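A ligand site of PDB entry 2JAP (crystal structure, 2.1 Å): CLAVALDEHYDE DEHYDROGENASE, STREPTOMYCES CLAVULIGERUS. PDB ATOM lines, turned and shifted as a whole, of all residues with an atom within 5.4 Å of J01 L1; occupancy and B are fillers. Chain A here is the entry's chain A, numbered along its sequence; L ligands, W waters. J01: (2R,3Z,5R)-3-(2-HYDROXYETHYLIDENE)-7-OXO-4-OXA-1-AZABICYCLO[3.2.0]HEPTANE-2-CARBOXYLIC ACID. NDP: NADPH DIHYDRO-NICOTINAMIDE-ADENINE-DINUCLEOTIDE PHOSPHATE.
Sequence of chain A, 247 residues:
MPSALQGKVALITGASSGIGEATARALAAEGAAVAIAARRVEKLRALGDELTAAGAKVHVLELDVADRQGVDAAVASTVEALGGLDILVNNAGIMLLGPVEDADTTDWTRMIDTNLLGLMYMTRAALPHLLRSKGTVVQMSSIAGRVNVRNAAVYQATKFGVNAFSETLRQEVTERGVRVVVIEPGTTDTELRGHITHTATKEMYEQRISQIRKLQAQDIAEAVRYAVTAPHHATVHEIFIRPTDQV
N of Leu 192 sits close to O3 of NDP L2. The guanidinium group (NH2) of Arg 208 lies within salt-bridge range of an oxygen (O4) of J01 L1, at 3.5 Å. An oxygen (O2D) of NDP L2 is in hydrogen-bond range of the side-chain hydroxyl (OH) of Tyr 155 (2.6 Å). The side-chain hydroxyl (OG1) of Thr 187 is in hydrogen-bond range of an oxygen (O5) of J01 L1, 2.6 Å away. OH of Tyr 205 is in hydrogen-bond range of O5 of J01 L1 (2.7 Å). The side-chain hydroxyl of Ser 142 is in hydrogen-bond range of an oxygen (O3) of J01 L1 (2.5 Å). The side-chain hydroxyl of Tyr 155 lies within hydrogen-bond range of an oxygen (O3) of J01 L1 (2.9 Å).
The backbone NH (N) of Val 149 lies within hydrogen-bond range of the side-chain amide oxygen (OE1) of Gln 156. N of Ile 143 lies within hydrogen-bond range of O of Pro 185. OG1 of Thr 187 is in hydrogen-bond range of NE2 of Gln 246 (2.9 Å). The side-chain amide nitrogen (NE2) of Gln 156 sits at hydrogen-bond distance from the backbone carbonyl oxygen (O) of Ala 152 (3.2 Å). OG of Ser 142 lies close to N of Ala 144, 2.9 Å away.
SD of Met 95 touches C6 of J01 L1, at 3.5 Å. Leu 97 touches J01 L1. CG2 of Ile 143 touches O4 of J01 L1 (3.6 Å). CB of Ala 144 touches O1 of J01 L1, 3.5 Å away. Val 149 touches J01 L1 (CG2 to O2, 3.8 Å). CB of Ala 152 touches C4 of J01 L1, 3.5 Å away. Gln 156 touches J01 L1 (OE1 to C4, 3.6 Å). Leu 192 touches J01 L1 (CD2 to C7, 3.8 Å). Hydrophobic or aromatic side chains within 4 Å of J01 L1: Met 95, Leu 97, Ile 143, Ala 144, Val 149, Ala 152, Tyr 155, Leu 192 and Tyr 205. Along chain A the residues within 4 Å of J01 L1 span positions 95 to 208. The nearest printed residue that does not touch J01 L1 is Ile 209 (4.2 Å).
Water W2 lies within hydrogen-bond range of an oxygen (O4) of J01 L1 and the guanidinium group of Arg 208.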
ATOM      1  N   MET A  95     -27.627  -1.966   5.569  1.00  0.00           N
ATOM      2  CA  MET A  95     -26.546  -1.746   6.507  1.00  0.00           C
ATOM      3  C   MET A  95     -26.544  -0.296   6.987  1.00  0.00           C
ATOM      4  O   MET A  95     -26.139   0.611   6.269  1.00  0.00           O
ATOM      5  CB  MET A  95     -25.194  -2.102   5.896  1.00  0.00           C
ATOM      6  CG  MET A  95     -24.044  -1.916   6.868  1.00  0.00           C
ATOM      7  SD  MET A  95     -22.437  -2.299   6.191  1.00  0.00           S
ATOM      8  CE  MET A  95     -22.212  -0.889   5.096  1.00  0.00           C
ATOM      9  N   LEU A  97     -24.967   1.985   9.584  1.00  0.00           N
ATOM     10  CA  LEU A  97     -23.846   2.109  10.512  1.00  0.00           C
ATOM     11  C   LEU A  97     -23.935   3.354  11.369  1.00  0.00           C
ATOM     12  O   LEU A  97     -24.529   4.352  10.970  1.00  0.00           O
ATOM     13  CB  LEU A  97     -22.528   2.120   9.723  1.00  0.00           C
ATOM     14  CG  LEU A  97     -22.257   0.923   8.802  1.00  0.00           C
ATOM     15  CD1 LEU A  97     -20.875   1.020   8.183  1.00  0.00           C
ATOM     16  CD2 LEU A  97     -22.412  -0.396   9.561  1.00  0.00           C
ATOM     17  N   SER A 142     -22.350 -11.905   6.001  1.00  0.00           N
ATOM     18  CA  SER A 142     -21.348 -10.893   5.854  1.00  0.00           C
ATOM     19  C   SER A 142     -20.133 -11.259   6.707  1.00  0.00           C
ATOM     20  O   SER A 142     -20.239 -12.085   7.625  1.00  0.00           O
ATOM     21  CB  SER A 142     -21.939  -9.544   6.333  1.00  0.00           C
ATOM     22  OG  SER A 142     -20.969  -8.524   6.334  1.00  0.00           O
ATOM     23  N   ILE A 143     -19.008 -10.613   6.414  1.00  0.00           N
ATOM     24  CA  ILE A 143     -17.869 -10.540   7.342  1.00  0.00           C
ATOM     25  C   ILE A 143     -18.371 -10.064   8.709  1.00  0.00           C
ATOM     26  O   ILE A 143     -17.832 -10.443   9.740  1.00  0.00           O
ATOM     27  CB  ILE A 143     -16.722  -9.606   6.803  1.00  0.00           C
ATOM     28  CG1 ILE A 143     -15.497  -9.603   7.749  1.00  0.00           C
ATOM     29  CG2 ILE A 143     -17.250  -8.157   6.490  1.00  0.00           C
ATOM     30  CD1 ILE A 143     -14.208  -9.048   7.131  1.00  0.00           C
ATOM     31  N   ALA A 144     -19.440  -9.260   8.693  1.00  0.00           N
ATOM     32  CA  ALA A 144     -20.114  -8.753   9.894  1.00  0.00           C
ATOM     33  C   ALA A 144     -20.819  -9.833  10.714  1.00  0.00           C
ATOM     34  O   ALA A 144     -21.271  -9.565  11.814  1.00  0.00           O
ATOM     35  CB  ALA A 144     -21.092  -7.636   9.525  1.00  0.00           C
ATOM     36  N   VAL A 149     -16.491  -4.986  14.268  1.00  0.00           N
ATOM     37  CA  VAL A 149     -15.779  -3.699  14.294  1.00  0.00           C
ATOM     38  C   VAL A 149     -16.688  -2.591  14.818  1.00  0.00           C
ATOM     39  O   VAL A 149     -17.915  -2.759  14.846  1.00  0.00           O
ATOM     40  CB  VAL A 149     -15.203  -3.294  12.885  1.00  0.00           C
ATOM     41  CG1 VAL A 149     -14.193  -4.318  12.389  1.00  0.00           C
ATOM     42  CG2 VAL A 149     -16.326  -3.101  11.877  1.00  0.00           C
ATOM     43  N   ARG A 150     -16.097  -1.460  15.213  1.00  0.00           N
ATOM     44  CA  ARG A 150     -16.845  -0.340  15.785  1.00  0.00           C
ATOM     45  C   ARG A 150     -17.857   0.250  14.806  1.00  0.00           C
ATOM     46  O   ARG A 150     -17.663   0.220  13.591  1.00  0.00           O
ATOM     47  CB  ARG A 150     -15.914   0.781  16.271  1.00  0.00           C
ATOM     48  CG  ARG A 150     -14.966   0.369  17.384  1.00  0.00           C
ATOM     49  CD  ARG A 150     -14.148   1.552  17.859  1.00  0.00           C
ATOM     50  NE  ARG A 150     -12.727   1.286  17.739  1.00  0.00           N
ATOM     51  CZ  ARG A 150     -11.780   1.996  18.352  1.00  0.00           C
ATOM     52  NH1 ARG A 150     -12.102   3.015  19.149  1.00  0.00           N
ATOM     53  NH2 ARG A 150     -10.499   1.673  18.176  1.00  0.00           N
ATOM     54  N   ALA A 152     -20.872  -0.739  14.027  1.00  0.00           N
ATOM     55  CA  ALA A 152     -21.696  -1.669  13.280  1.00  0.00           C
ATOM     56  C   ALA A 152     -22.391  -2.670  14.212  1.00  0.00           C
ATOM     57  O   ALA A 152     -22.687  -3.788  13.797  1.00  0.00           O
ATOM     58  CB  ALA A 152     -20.869  -2.392  12.238  1.00  0.00           C
ATOM     59  N   TYR A 155     -25.979  -3.989  13.110  1.00  0.00           N
ATOM     60  CA  TYR A 155     -25.778  -4.686  11.837  1.00  0.00           C
ATOM     61  C   TYR A 155     -25.099  -6.040  12.066  1.00  0.00           C
ATOM     62  O   TYR A 155     -25.588  -7.080  11.600  1.00  0.00           O
ATOM     63  CB  TYR A 155     -24.951  -3.827  10.868  1.00  0.00           C
ATOM     64  CG  TYR A 155     -24.755  -4.465   9.503  1.00  0.00           C
ATOM     65  CD1 TYR A 155     -25.841  -4.660   8.634  1.00  0.00           C
ATOM     66  CD2 TYR A 155     -23.487  -4.879   9.074  1.00  0.00           C
ATOM     67  CE1 TYR A 155     -25.674  -5.247   7.383  1.00  0.00           C
ATOM     68  CE2 TYR A 155     -23.313  -5.454   7.822  1.00  0.00           C
ATOM     69  CZ  TYR A 155     -24.409  -5.641   6.980  1.00  0.00           C
ATOM     70  OH  TYR A 155     -24.260  -6.216   5.741  1.00  0.00           O
ATOM     71  N   GLN A 156     -23.992  -6.015  12.814  1.00  0.00           N
ATOM     72  CA  GLN A 156     -23.293  -7.244  13.193  1.00  0.00           C
ATOM     73  C   GLN A 156     -24.173  -8.187  13.998  1.00  0.00           C
ATOM     74  O   GLN A 156     -24.109  -9.404  13.792  1.00  0.00           O
ATOM     75  CB  GLN A 156     -21.985  -6.918  13.919  1.00  0.00           C
ATOM     76  CG  GLN A 156     -20.941  -6.444  12.903  1.00  0.00           C
ATOM     77  CD  GLN A 156     -19.846  -5.541  13.420  1.00  0.00           C
ATOM     78  OE1 GLN A 156     -18.925  -5.264  12.679  1.00  0.00           O
ATOM     79  NE2 GLN A 156     -19.928  -5.090  14.683  1.00  0.00           N
ATOM     80  N   PRO A 185     -19.497 -12.207   2.487  1.00  0.00           N
ATOM     81  CA  PRO A 185     -18.611 -11.271   1.810  1.00  0.00           C
ATOM     82  C   PRO A 185     -18.031 -10.212   2.741  1.00  0.00           C
ATOM     83  O   PRO A 185     -18.688  -9.780   3.687  1.00  0.00           O
ATOM     84  CB  PRO A 185     -19.528 -10.601   0.776  1.00  0.00           C
ATOM     85  CG  PRO A 185     -20.808 -11.376   0.772  1.00  0.00           C
ATOM     86  CD  PRO A 185     -20.919 -11.959   2.160  1.00  0.00           C
ATOM     87  N   GLY A 186     -16.789  -9.809   2.466  1.00  0.00           N
ATOM     88  CA  GLY A 186     -16.241  -8.571   2.968  1.00  0.00           C
ATOM     89  C   GLY A 186     -16.707  -7.450   2.061  1.00  0.00           C
ATOM     90  O   GLY A 186     -17.640  -7.625   1.265  1.00  0.00           O
ATOM     91  N   THR A 187     -16.042  -6.301   2.150  1.00  0.00           N
ATOM     92  CA  THR A 187     -16.425  -5.103   1.414  1.00  0.00           C
ATOM     93  C   THR A 187     -16.633  -5.352  -0.081  1.00  0.00           C
ATOM     94  O   THR A 187     -15.704  -5.727  -0.804  1.00  0.00           O
ATOM     95  CB  THR A 187     -15.379  -3.995   1.593  1.00  0.00           C
ATOM     96  OG1 THR A 187     -14.983  -3.944   2.975  1.00  0.00           O
ATOM     97  CG2 THR A 187     -15.973  -2.667   1.163  1.00  0.00           C
ATOM     98  N   LEU A 192     -25.284  -0.587  -1.134  1.00  0.00           N
ATOM     99  CA  LEU A 192     -25.520  -0.804   0.308  1.00  0.00           C
ATOM    100  C   LEU A 192     -25.190   0.398   1.206  1.00  0.00           C
ATOM    101  O   LEU A 192     -26.027   0.813   2.026  1.00  0.00           O
ATOM    102  CB  LEU A 192     -24.764  -2.053   0.805  1.00  0.00           C
ATOM    103  CG  LEU A 192     -25.107  -2.621   2.198  1.00  0.00           C
ATOM    104  CD1 LEU A 192     -26.424  -3.400   2.186  1.00  0.00           C
ATOM    105  CD2 LEU A 192     -23.996  -3.500   2.772  1.00  0.00           C
ATOM    106  N   TYR A 205     -16.709   5.329   7.093  1.00  0.00           N
ATOM    107  CA  TYR A 205     -16.722   4.050   6.386  1.00  0.00           C
ATOM    108  C   TYR A 205     -16.215   4.198   4.948  1.00  0.00           C
ATOM    109  O   TYR A 205     -15.406   3.379   4.486  1.00  0.00           O
ATOM    110  CB  TYR A 205     -18.131   3.426   6.438  1.00  0.00           C
ATOM    111  CG  TYR A 205     -18.256   2.124   5.687  1.00  0.00           C
ATOM    112  CD1 TYR A 205     -17.588   0.974   6.121  1.00  0.00           C
ATOM    113  CD2 TYR A 205     -19.051   2.032   4.531  1.00  0.00           C
ATOM    114  CE1 TYR A 205     -17.699  -0.232   5.430  1.00  0.00           C
ATOM    115  CE2 TYR A 205     -19.171   0.829   3.826  1.00  0.00           C
ATOM    116  CZ  TYR A 205     -18.493  -0.299   4.278  1.00  0.00           C
ATOM    117  OH  TYR A 205     -18.595  -1.486   3.593  1.00  0.00           O
ATOM    118  N   ARG A 208     -12.534   4.492   4.968  1.00  0.00           N
ATOM    119  CA  ARG A 208     -11.980   3.192   5.372  1.00  0.00           C
ATOM    120  C   ARG A 208     -11.805   2.234   4.193  1.00  0.00           C
ATOM    121  O   ARG A 208     -10.768   1.556   4.071  1.00  0.00           O
ATOM    122  CB  ARG A 208     -12.892   2.526   6.422  1.00  0.00           C
ATOM    123  CG  ARG A 208     -12.465   1.105   6.865  1.00  0.00           C
ATOM    124  CD  ARG A 208     -13.594   0.286   7.519  1.00  0.00           C
ATOM    125  NE  ARG A 208     -13.213  -1.135   7.611  1.00  0.00           N
ATOM    126  CZ  ARG A 208     -13.969  -2.123   8.077  1.00  0.00           C
ATOM    127  NH1 ARG A 208     -15.201  -1.890   8.528  1.00  0.00           N
ATOM    128  NH2 ARG A 208     -13.489  -3.354   8.100  1.00  0.00           N
ATOM    129  N   ILE A 209     -12.821   2.188   3.330  1.00  0.00           N
ATOM    130  CA  ILE A 209     -12.842   1.276   2.181  1.00  0.00           C
ATOM    131  C   ILE A 209     -12.350   1.898   0.858  1.00  0.00           C
ATOM    132  O   ILE A 209     -12.365   1.246  -0.185  1.00  0.00           O
ATOM    133  CB  ILE A 209     -14.256   0.626   2.016  1.00  0.00           C
ATOM    134  CG1 ILE A 209     -15.329   1.690   1.735  1.00  0.00           C
ATOM    135  CG2 ILE A 209     -14.625  -0.200   3.281  1.00  0.00           C
ATOM    136  CD1 ILE A 209     -16.677   1.116   1.314  1.00  0.00           C
ATOM    137  N   GLN A 246      -7.434  -5.978   2.250  1.00  0.00           N
ATOM    138  CA  GLN A 246      -7.985  -5.563   3.536  1.00  0.00           C
ATOM    139  C   GLN A 246      -7.568  -6.453   4.715  1.00  0.00           C
ATOM    140  O   GLN A 246      -7.955  -7.611   4.778  1.00  0.00           O
ATOM    141  CB  GLN A 246      -9.517  -5.517   3.436  1.00  0.00           C
ATOM    142  CG  GLN A 246     -10.221  -4.896   4.636  1.00  0.00           C
ATOM    143  CD  GLN A 246     -11.716  -5.032   4.544  1.00  0.00           C
ATOM    144  OE1 GLN A 246     -12.276  -6.089   4.832  1.00  0.00           O
ATOM    145  NE2 GLN A 246     -12.377  -3.946   4.161  1.00  0.00           N
HETATM  146  O2  J01 L   1     -18.665  -1.889   9.107  1.00  0.00           O
HETATM  147  C5  J01 L   1     -18.759  -3.087   8.865  1.00  0.00           C
HETATM  148  C4  J01 L   1     -19.693  -4.115   9.400  1.00  0.00           C
HETATM  149  C3  J01 L   1     -18.989  -4.980   8.356  1.00  0.00           C
HETATM  150  N1  J01 L   1     -18.043  -3.903   7.979  1.00  0.00           N
HETATM  151  O1  J01 L   1     -19.845  -5.277   7.250  1.00  0.00           O
HETATM  152  C1  J01 L   1     -19.391  -4.433   6.157  1.00  0.00           C
HETATM  153  C2  J01 L   1     -18.248  -3.569   6.552  1.00  0.00           C
HETATM  154  C8  J01 L   1     -17.038  -3.906   5.742  1.00  0.00           C
HETATM  155  O5  J01 L   1     -16.950  -3.383   4.602  1.00  0.00           O
HETATM  156  O4  J01 L   1     -16.187  -4.689   6.232  1.00  0.00           O
HETATM  157  C6  J01 L   1     -19.900  -4.392   4.917  1.00  0.00           C
HETATM  158  C7  J01 L   1     -21.069  -5.193   4.436  1.00  0.00           C
HETATM  159  O3  J01 L   1     -21.436  -6.252   5.315  1.00  0.00           O
HETATM  160  PA  NDP L   2     -27.779  -3.197  -2.249  1.00  0.00           P
HETATM  161  O1A NDP L   2     -28.387  -2.078  -1.481  1.00  0.00           O
HETATM  162  O2A NDP L   2     -27.372  -2.801  -3.627  1.00  0.00           O
HETATM  163  O5B NDP L   2     -28.824  -4.410  -2.330  1.00  0.00           O
HETATM  164  C5B NDP L   2     -29.784  -4.606  -1.314  1.00  0.00           C
HETATM  165  C4B NDP L   2     -30.996  -5.208  -1.992  1.00  0.00           C
HETATM  166  O4B NDP L   2     -31.992  -5.520  -1.035  1.00  0.00           O
HETATM  167  C3B NDP L   2     -31.595  -4.212  -2.946  1.00  0.00           C
HETATM  168  O3B NDP L   2     -31.969  -4.936  -4.107  1.00  0.00           O
HETATM  169  C2B NDP L   2     -32.828  -3.685  -2.237  1.00  0.00           C
HETATM  170  O2B NDP L   2     -33.795  -3.454  -3.223  1.00  0.00           O
HETATM  171  C1B NDP L   2     -33.211  -4.885  -1.399  1.00  0.00           C
HETATM  172  N9A NDP L   2     -33.988  -4.604  -0.183  1.00  0.00           N
HETATM  173  C8A NDP L   2     -33.683  -3.795   0.873  1.00  0.00           C
HETATM  174  N7A NDP L   2     -34.687  -3.879   1.789  1.00  0.00           N
HETATM  175  C5A NDP L   2     -35.619  -4.746   1.323  1.00  0.00           C
HETATM  176  C6A NDP L   2     -36.830  -5.216   1.841  1.00  0.00           C
HETATM  177  N6A NDP L   2     -37.281  -4.786   3.016  1.00  0.00           N
HETATM  178  N1A NDP L   2     -37.569  -6.133   1.117  1.00  0.00           N
HETATM  179  C2A NDP L   2     -37.114  -6.586  -0.111  1.00  0.00           C
HETATM  180  N3A NDP L   2     -35.924  -6.112  -0.624  1.00  0.00           N
HETATM  181  C4A NDP L   2     -35.182  -5.213   0.088  1.00  0.00           C
HETATM  182  O3  NDP L   2     -26.550  -3.763  -1.373  1.00  0.00           O
HETATM  183  PN  NDP L   2     -25.912  -5.246  -1.450  1.00  0.00           P
HETATM  184  O1N NDP L   2     -24.515  -5.114  -0.962  1.00  0.00           O
HETATM  185  O2N NDP L   2     -26.176  -5.860  -2.770  1.00  0.00           O
HETATM  186  O5D NDP L   2     -26.724  -5.980  -0.282  1.00  0.00           O
HETATM  187  C5D NDP L   2     -27.274  -7.265  -0.437  1.00  0.00           C
HETATM  188  C4D NDP L   2     -26.841  -8.148   0.727  1.00  0.00           C
HETATM  189  O4D NDP L   2     -25.432  -8.247   0.744  1.00  0.00           O
HETATM  190  C3D NDP L   2     -27.255  -7.615   2.097  1.00  0.00           C
HETATM  191  O3D NDP L   2     -27.789  -8.664   2.876  1.00  0.00           O
HETATM  192  C2D NDP L   2     -25.955  -7.158   2.715  1.00  0.00           C
HETATM  193  O2D NDP L   2     -25.982  -7.185   4.127  1.00  0.00           O
HETATM  194  C1D NDP L   2     -25.028  -8.187   2.097  1.00  0.00           C
HETATM  195  N1N NDP L   2     -23.611  -7.835   2.211  1.00  0.00           N
HETATM  196  C2N NDP L   2     -23.088  -6.745   1.547  1.00  0.00           C
HETATM  197  C3N NDP L   2     -21.716  -6.490   1.572  1.00  0.00           C
HETATM  198  C7N NDP L   2     -21.154  -5.297   0.855  1.00  0.00           C
HETATM  199  O7N NDP L   2     -19.918  -4.758   1.277  1.00  0.00           O
HETATM  200  N7N NDP L   2     -21.818  -4.767  -0.169  1.00  0.00           N
HETATM  201  C4N NDP L   2     -20.767  -7.386   2.306  1.00  0.00           C
HETATM  202  C5N NDP L   2     -21.458  -8.526   2.998  1.00  0.00           C
HETATM  203  C6N NDP L   2     -22.832  -8.712   2.916  1.00  0.00           C
HETATM  204  P2B NDP L   2     -35.110  -2.557  -3.015  1.00  0.00           P
HETATM  205  O1X NDP L   2     -35.672  -2.411  -4.405  1.00  0.00           O
HETATM  206  O2X NDP L   2     -36.079  -3.271  -2.118  1.00  0.00           O
HETATM  207  O3X NDP L   2     -34.749  -1.220  -2.388  1.00  0.00           O
HETATM  208  O   HOH W   1     -17.392  -6.584  10.441  1.00  0.00           O
HETATM  209  O   HOH W   2     -15.485  -5.590   8.760  1.00  0.00           O
